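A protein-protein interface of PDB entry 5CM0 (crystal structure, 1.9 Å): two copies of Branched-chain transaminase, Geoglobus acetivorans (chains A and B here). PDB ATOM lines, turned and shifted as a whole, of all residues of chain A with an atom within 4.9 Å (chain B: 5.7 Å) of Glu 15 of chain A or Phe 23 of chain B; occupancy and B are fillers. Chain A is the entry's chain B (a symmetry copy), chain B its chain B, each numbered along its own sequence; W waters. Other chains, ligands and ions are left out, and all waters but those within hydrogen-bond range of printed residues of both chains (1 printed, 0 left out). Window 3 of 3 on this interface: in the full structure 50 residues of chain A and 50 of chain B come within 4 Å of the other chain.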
ATOM      1  N   GLU A   3      11.856 -10.466  -4.807  1.00  0.00           N
ATOM      2  CA  GLU A   3      10.894 -11.238  -5.660  1.00  0.00           C
ATOM      3  C   GLU A   3       9.521 -10.577  -5.577  1.00  0.00           C
ATOM      4  O   GLU A   3       9.071 -10.233  -4.485  1.00  0.00           O
ATOM      5  CB  GLU A   3      10.808 -12.673  -5.172  1.00  0.00           C
ATOM      6  CG  GLU A   3      10.428 -13.647  -6.246  1.00  0.00           C
ATOM      7  CD  GLU A   3      10.342 -15.067  -5.760  1.00  0.00           C
ATOM      8  OE1 GLU A   3      10.548 -15.298  -4.561  1.00  0.00           O
ATOM      9  OE2 GLU A   3      10.054 -15.960  -6.579  1.00  0.00           O
ATOM     10  N   LEU A   4       8.834 -10.374  -6.703  1.00  0.00           N
ATOM     11  CA  LEU A   4       7.459  -9.822  -6.632  1.00  0.00           C
ATOM     12  C   LEU A   4       6.506 -10.732  -5.884  1.00  0.00           C
ATOM     13  O   LEU A   4       6.643 -11.986  -5.871  1.00  0.00           O
ATOM     14  CB  LEU A   4       6.940  -9.561  -8.032  1.00  0.00           C
ATOM     15  CG  LEU A   4       7.679  -8.494  -8.835  1.00  0.00           C
ATOM     16  CD1 LEU A   4       7.302  -8.660 -10.309  1.00  0.00           C
ATOM     17  CD2 LEU A   4       7.353  -7.112  -8.281  1.00  0.00           C
ATOM     18  N   LEU A   5       5.548 -10.113  -5.196  1.00  0.00           N
ATOM     19  CA  LEU A   5       4.539 -10.852  -4.452  1.00  0.00           C
ATOM     20  C   LEU A   5       3.241 -10.866  -5.281  1.00  0.00           C
ATOM     21  O   LEU A   5       2.895  -9.858  -5.920  1.00  0.00           O
ATOM     22  CB  LEU A   5       4.273 -10.190  -3.101  1.00  0.00           C
ATOM     23  CG  LEU A   5       5.466 -10.182  -2.106  1.00  0.00           C
ATOM     24  CD1 LEU A   5       5.192  -9.229  -0.973  1.00  0.00           C
ATOM     25  CD2 LEU A   5       5.735 -11.561  -1.567  1.00  0.00           C
ATOM     26  N   VAL A   6       2.551 -11.991  -5.191  1.00  0.00           N
ATOM     27  CA  VAL A   6       1.209 -12.208  -5.763  1.00  0.00           C
ATOM     28  C   VAL A   6       0.169 -12.294  -4.648  1.00  0.00           C
ATOM     29  O   VAL A   6       0.297 -13.137  -3.743  1.00  0.00           O
ATOM     30  CB  VAL A   6       1.185 -13.561  -6.527  1.00  0.00           C
ATOM     31  CG1 VAL A   6      -0.217 -13.835  -7.132  1.00  0.00           C
ATOM     32  CG2 VAL A   6       2.235 -13.581  -7.620  1.00  0.00           C
ATOM     33  N   VAL A  13       2.273 -13.785  -1.725  1.00  0.00           N
ATOM     34  CA  VAL A  13       3.063 -14.978  -1.923  1.00  0.00           C
ATOM     35  C   VAL A  13       4.085 -14.664  -2.987  1.00  0.00           C
ATOM     36  O   VAL A  13       3.731 -14.130  -4.065  1.00  0.00           O
ATOM     37  CB  VAL A  13       2.164 -16.148  -2.370  1.00  0.00           C
ATOM     38  CG1 VAL A  13       2.955 -17.428  -2.620  1.00  0.00           C
ATOM     39  CG2 VAL A  13       1.063 -16.349  -1.369  1.00  0.00           C
ATOM     40  N   PRO A  14       5.368 -15.006  -2.719  1.00  0.00           N
ATOM     41  CA  PRO A  14       6.342 -14.784  -3.778  1.00  0.00           C
ATOM     42  C   PRO A  14       5.928 -15.521  -5.070  1.00  0.00           C
ATOM     43  O   PRO A  14       5.395 -16.634  -5.030  1.00  0.00           O
ATOM     44  CB  PRO A  14       7.648 -15.372  -3.201  1.00  0.00           C
ATOM     45  CG  PRO A  14       7.399 -15.549  -1.754  1.00  0.00           C
ATOM     46  CD  PRO A  14       5.926 -15.845  -1.649  1.00  0.00           C
ATOM     47  N   GLU A  15       6.175 -14.868  -6.189  1.00  0.00           N
ATOM     48  CA  GLU A  15       5.817 -15.358  -7.516  1.00  0.00           C
ATOM     49  C   GLU A  15       6.061 -16.804  -7.685  1.00  0.00           C
ATOM     50  O   GLU A  15       5.175 -17.526  -8.078  1.00  0.00           O
ATOM     51  CB  GLU A  15       6.692 -14.711  -8.547  1.00  0.00           C
ATOM     52  CG  GLU A  15       6.322 -13.314  -8.863  1.00  0.00           C
ATOM     53  CD  GLU A  15       6.949 -12.926 -10.145  1.00  0.00           C
ATOM     54  OE1 GLU A  15       8.089 -13.354 -10.415  1.00  0.00           O
ATOM     55  OE2 GLU A  15       6.309 -12.184 -10.864  1.00  0.00           O
ATOM     56  N   SER A  16       7.274 -17.231  -7.359  1.00  0.00           N
ATOM     57  CA  SER A  16       7.714 -18.593  -7.623  1.00  0.00           C
ATOM     58  C   SER A  16       6.992 -19.590  -6.751  1.00  0.00           C
ATOM     59  O   SER A  16       7.025 -20.784  -7.038  1.00  0.00           O
ATOM     60  CB  SER A  16       9.241 -18.725  -7.443  1.00  0.00           C
ATOM     61  OG  SER A  16       9.609 -18.373  -6.107  1.00  0.00           O
ATOM     62  N   GLN A  17       6.332 -19.127  -5.694  1.00  0.00           N
ATOM     63  CA  GLN A  17       5.549 -19.993  -4.852  1.00  0.00           C
ATOM     64  C   GLN A  17       4.030 -19.836  -5.111  1.00  0.00           C
ATOM     65  O   GLN A  17       3.193 -20.579  -4.507  1.00  0.00           O
ATOM     66  CB  GLN A  17       5.937 -19.717  -3.382  1.00  0.00           C
ATOM     67  N   ALA A  18       3.664 -18.902  -6.001  1.00  0.00           N
ATOM     68  CA  ALA A  18       2.260 -18.589  -6.259  1.00  0.00           C
ATOM     69  C   ALA A  18       1.646 -19.660  -7.195  1.00  0.00           C
ATOM     70  O   ALA A  18       1.816 -19.612  -8.402  1.00  0.00           O
ATOM     71  CB  ALA A  18       2.125 -17.204  -6.860  1.00  0.00           C
ATOM     72  N   ILE A 116      -2.127 -10.472  -9.834  1.00  0.00           N
ATOM     73  CA  ILE A 116      -0.769 -10.482 -10.350  1.00  0.00           C
ATOM     74  C   ILE A 116      -0.446  -9.070 -10.716  1.00  0.00           C
ATOM     75  O   ILE A 116      -1.274  -8.380 -11.327  1.00  0.00           O
ATOM     76  CB  ILE A 116      -0.634 -11.424 -11.577  1.00  0.00           C
ATOM     77  CG1 ILE A 116      -0.805 -12.876 -11.148  1.00  0.00           C
ATOM     78  CG2 ILE A 116       0.705 -11.214 -12.315  1.00  0.00           C
ATOM     79  CD1 ILE A 116      -0.978 -13.863 -12.293  1.00  0.00           C
ATOM     80  N   LYS A 118       2.867  -6.833 -12.453  1.00  0.00           N
ATOM     81  CA  LYS A 118       4.131  -7.007 -13.146  1.00  0.00           C
ATOM     82  C   LYS A 118       4.562  -5.680 -13.663  1.00  0.00           C
ATOM     83  O   LYS A 118       3.715  -4.926 -14.125  1.00  0.00           O
ATOM     84  CB  LYS A 118       3.991  -7.929 -14.349  1.00  0.00           C
ATOM     85  CG  LYS A 118       3.974  -9.401 -14.025  1.00  0.00           C
ATOM     86  CD  LYS A 118       5.371  -9.953 -13.789  1.00  0.00           C
ATOM     87  CE  LYS A 118       5.349 -11.469 -13.889  1.00  0.00           C
ATOM     88  NZ  LYS A 118       6.636 -12.133 -13.567  1.00  0.00           N
ATOM     89  N   SER B  21       1.684 -23.362 -11.155  1.00  0.00           N
ATOM     90  CA  SER B  21       1.912 -21.950 -11.152  1.00  0.00           C
ATOM     91  C   SER B  21       0.745 -21.155 -11.732  1.00  0.00           C
ATOM     92  O   SER B  21       0.205 -21.549 -12.753  1.00  0.00           O
ATOM     93  CB  SER B  21       3.133 -21.655 -11.971  1.00  0.00           C
ATOM     94  OG  SER B  21       3.294 -20.271 -12.139  1.00  0.00           O
ATOM     95  N   VAL B  22       0.415 -20.023 -11.105  1.00  0.00           N
ATOM     96  CA  VAL B  22      -0.622 -19.132 -11.612  1.00  0.00           C
ATOM     97  C   VAL B  22      -0.258 -18.538 -13.002  1.00  0.00           C
ATOM     98  O   VAL B  22      -1.126 -17.980 -13.692  1.00  0.00           O
ATOM     99  CB  VAL B  22      -0.978 -17.988 -10.633  1.00  0.00           C
ATOM    100  CG1 VAL B  22      -1.637 -18.496  -9.349  1.00  0.00           C
ATOM    101  CG2 VAL B  22       0.232 -17.141 -10.311  1.00  0.00           C
ATOM    102  N   PHE B  23       1.012 -18.626 -13.386  1.00  0.00           N
ATOM    103  CA  PHE B  23       1.481 -18.201 -14.709  1.00  0.00           C
ATOM    104  C   PHE B  23       1.395 -19.260 -15.799  1.00  0.00           C
ATOM    105  O   PHE B  23       1.665 -18.951 -16.952  1.00  0.00           O
ATOM    106  CB  PHE B  23       2.923 -17.706 -14.599  1.00  0.00           C
ATOM    107  CG  PHE B  23       3.063 -16.551 -13.645  1.00  0.00           C
ATOM    108  CD1 PHE B  23       2.830 -15.296 -14.071  1.00  0.00           C
ATOM    109  CD2 PHE B  23       3.367 -16.763 -12.291  1.00  0.00           C
ATOM    110  CE1 PHE B  23       2.940 -14.212 -13.195  1.00  0.00           C
ATOM    111  CE2 PHE B  23       3.497 -15.678 -11.416  1.00  0.00           C
ATOM    112  CZ  PHE B  23       3.247 -14.413 -11.869  1.00  0.00           C
ATOM    113  N   ASP B  24       1.052 -20.499 -15.445  1.00  0.00           N
ATOM    114  CA  ASP B  24       0.814 -21.570 -16.437  1.00  0.00           C
ATOM    115  C   ASP B  24      -0.363 -21.082 -17.372  1.00  0.00           C
ATOM    116  O   ASP B  24      -1.406 -20.661 -16.897  1.00  0.00           O
ATOM    117  CB  ASP B  24       0.444 -22.846 -15.711  1.00  0.00           C
ATOM    118  CG  ASP B  24       0.386 -24.064 -16.630  1.00  0.00           C
ATOM    119  OD1 ASP B  24      -0.099 -23.998 -17.771  1.00  0.00           O
ATOM    120  OD2 ASP B  24       0.902 -25.105 -16.262  1.00  0.00           O
ATOM    121  N   HIS B  25      -0.152 -21.045 -18.661  1.00  0.00           N
ATOM    122  CA  HIS B  25      -1.227 -20.639 -19.576  1.00  0.00           C
ATOM    123  C   HIS B  25      -2.453 -21.552 -19.538  1.00  0.00           C
ATOM    124  O   HIS B  25      -3.527 -21.135 -20.017  1.00  0.00           O
ATOM    125  CB  HIS B  25      -0.685 -20.503 -20.977  1.00  0.00           C
ATOM    126  CG  HIS B  25       0.107 -19.261 -21.194  1.00  0.00           C
ATOM    127  ND1 HIS B  25       0.290 -18.703 -22.439  1.00  0.00           N
ATOM    128  CD2 HIS B  25       0.773 -18.467 -20.321  1.00  0.00           C
ATOM    129  CE1 HIS B  25       1.022 -17.611 -22.329  1.00  0.00           C
ATOM    130  NE2 HIS B  25       1.312 -17.436 -21.050  1.00  0.00           N
ATOM    131  N   PHE B  27      -3.890 -22.330 -16.755  1.00  0.00           N
ATOM    132  CA  PHE B  27      -4.662 -21.565 -15.798  1.00  0.00           C
ATOM    133  C   PHE B  27      -5.120 -20.212 -16.325  1.00  0.00           C
ATOM    134  O   PHE B  27      -6.300 -19.877 -16.183  1.00  0.00           O
ATOM    135  CB  PHE B  27      -3.866 -21.377 -14.517  1.00  0.00           C
ATOM    136  CG  PHE B  27      -4.596 -20.622 -13.446  1.00  0.00           C
ATOM    137  CD1 PHE B  27      -5.688 -21.197 -12.814  1.00  0.00           C
ATOM    138  CD2 PHE B  27      -4.184 -19.363 -13.058  1.00  0.00           C
ATOM    139  CE1 PHE B  27      -6.329 -20.537 -11.796  1.00  0.00           C
ATOM    140  CE2 PHE B  27      -4.850 -18.682 -12.055  1.00  0.00           C
ATOM    141  CZ  PHE B  27      -5.921 -19.266 -11.435  1.00  0.00           C
ATOM    142  N   LEU B  28      -4.226 -19.435 -16.951  1.00  0.00           N
ATOM    143  CA  LEU B  28      -4.581 -18.104 -17.370  1.00  0.00           C
ATOM    144  C   LEU B  28      -5.612 -18.042 -18.534  1.00  0.00           C
ATOM    145  O   LEU B  28      -6.428 -17.111 -18.604  1.00  0.00           O
ATOM    146  CB  LEU B  28      -3.328 -17.357 -17.826  1.00  0.00           C
ATOM    147  CG  LEU B  28      -2.290 -16.970 -16.759  1.00  0.00           C
ATOM    148  CD1 LEU B  28      -1.117 -16.240 -17.397  1.00  0.00           C
ATOM    149  CD2 LEU B  28      -2.927 -16.086 -15.705  1.00  0.00           C
ATOM    150  N   GLY B  97       2.015 -24.577 -20.385  1.00  0.00           N
ATOM    151  CA  GLY B  97       3.028 -24.182 -19.421  1.00  0.00           C
ATOM    152  C   GLY B  97       3.098 -22.696 -19.263  1.00  0.00           C
ATOM    153  O   GLY B  97       2.273 -21.953 -19.805  1.00  0.00           O
ATOM    154  N   ALA B  98       4.083 -22.249 -18.485  1.00  0.00           N
ATOM    155  CA  ALA B  98       4.290 -20.823 -18.245  1.00  0.00           C
ATOM    156  C   ALA B  98       4.983 -20.129 -19.410  1.00  0.00           C
ATOM    157  O   ALA B  98       5.672 -20.754 -20.208  1.00  0.00           O
ATOM    158  CB  ALA B  98       5.027 -20.649 -16.938  1.00  0.00           C
ATOM    159  N   GLY B  99       4.709 -18.835 -19.585  1.00  0.00           N
ATOM    160  CA  GLY B  99       5.298 -18.074 -20.685  1.00  0.00           C
ATOM    161  C   GLY B  99       5.540 -16.610 -20.322  1.00  0.00           C
ATOM    162  O   GLY B  99       6.043 -16.315 -19.250  1.00  0.00           O
ATOM    163  N   ASP B 100       5.190 -15.679 -21.204  1.00  0.00           N
ATOM    164  CA  ASP B 100       4.965 -14.324 -20.728  1.00  0.00           C
ATOM    165  C   ASP B 100       3.487 -14.245 -20.347  1.00  0.00           C
ATOM    166  O   ASP B 100       2.686 -15.179 -20.525  1.00  0.00           O
ATOM    167  CB  ASP B 100       5.502 -13.218 -21.682  1.00  0.00           C
ATOM    168  CG  ASP B 100       4.627 -12.935 -22.918  1.00  0.00           C
ATOM    169  OD1 ASP B 100       3.595 -13.577 -23.209  1.00  0.00           O
ATOM    170  OD2 ASP B 100       5.029 -12.019 -23.658  1.00  0.00           O
ATOM    171  N   LEU B 101       3.123 -13.116 -19.818  1.00  0.00           N
ATOM    172  CA  LEU B 101       1.806 -12.937 -19.368  1.00  0.00           C
ATOM    173  C   LEU B 101       0.816 -13.009 -20.537  1.00  0.00           C
ATOM    174  O   LEU B 101      -0.222 -13.665 -20.349  1.00  0.00           O
ATOM    175  CB  LEU B 101       1.680 -11.641 -18.567  1.00  0.00           C
ATOM    176  CG  LEU B 101       0.629 -11.592 -17.465  1.00  0.00           C
ATOM    177  CD1 LEU B 101       0.414 -12.887 -16.721  1.00  0.00           C
ATOM    178  CD2 LEU B 101       0.962 -10.491 -16.479  1.00  0.00           C
HETATM  179  O   HOH W   1       4.320 -19.390  -9.580  1.00  0.00           O
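Of chain B, only Phe 23 comes within 4 Å of Glu 15 of chain A. Printed residues of chain A within 4 Å of Phe 23 of chain B: Glu 15 (3.9 Å), Ile 116 (3.8 Å) and Lys 118 (3.7 Å). Of the printed residues of chain A, Val 22 of chain B touches Ala 18 (3.1 Å). Printed residues of chain A within 4 Å of Ser 21 of chain B: Ala 18. Of the printed residues of chain B, Ala 18 of chain A touches Ser 21 and Val 22. Printed residues of chain B within 4 Å of Lys 118 of chain A: Phe 23 (3.7 Å). Of the printed residues of chain B, Ile 116 of chain A touches Phe 23 (3.8 Å). Asp 100 of chain B touches none of the printed residues of chain A. The nearest residue of chain B that does not touch Glu 15 of chain A is Ser 21 of chain B (5.3 Å).
No position is printed for both chains. Of the 5 pairs that touch across the chains among the printed residues, none has its exchanged pair printed and touching as well.
OG of Ser 21 of chain B sits close to N of Phe 23 of chain B (3.1 Å). O of Leu 4 of chain A lies within hydrogen-bond range of N of Glu 15 of chain A (2.9 Å). OE2 of Glu 15 of chain A lies within salt-bridge range of NZ of Lys 118 of chain A (2.7 Å).
Among the printed residues, merely in contact across the chains: Ala 18 of chain A with Ser 21 of chain B (3.6 Å), Lys 118 of chain A with Phe 23 of chain B (3.7 Å), Ile 116 of chain A with Phe 23 of chain B (3.8 Å) and Glu 15 of chain A with Phe 23 of chain B (3.9 Å).
Hydrophobic or aromatic side chains of chain A that line the printed part of chain B: Ala 18 and Ile 116. Hydrophobic or aromatic side chains of chain B that line the printed part of chain A: Val 22 and Phe 23. Along chain B the printed residues that touch a printed residue of chain A span positions 21 to 23. Among the printed residues, 5 pairs touch across the chains. Among the printed residues, no Asp or Glu carboxylate lies within 4 Å of a Lys or Arg side-chain nitrogen of the other chain.
The backbone NH (N) of Val 22 of chain B is in hydrogen-bond range of the backbone carbonyl oxygen (O) of Ala 18 of chain A (3.1 Å).
Water W1 lies within hydrogen-bond range of the backbone carbonyl oxygen of Glu 15 of chain A (2.5 Å), the backbone carbonyl oxygen of Ala 18 of chain A (2.8 Å) and the side-chain hydroxyl of Ser 21 of chain B (2.9 Å).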
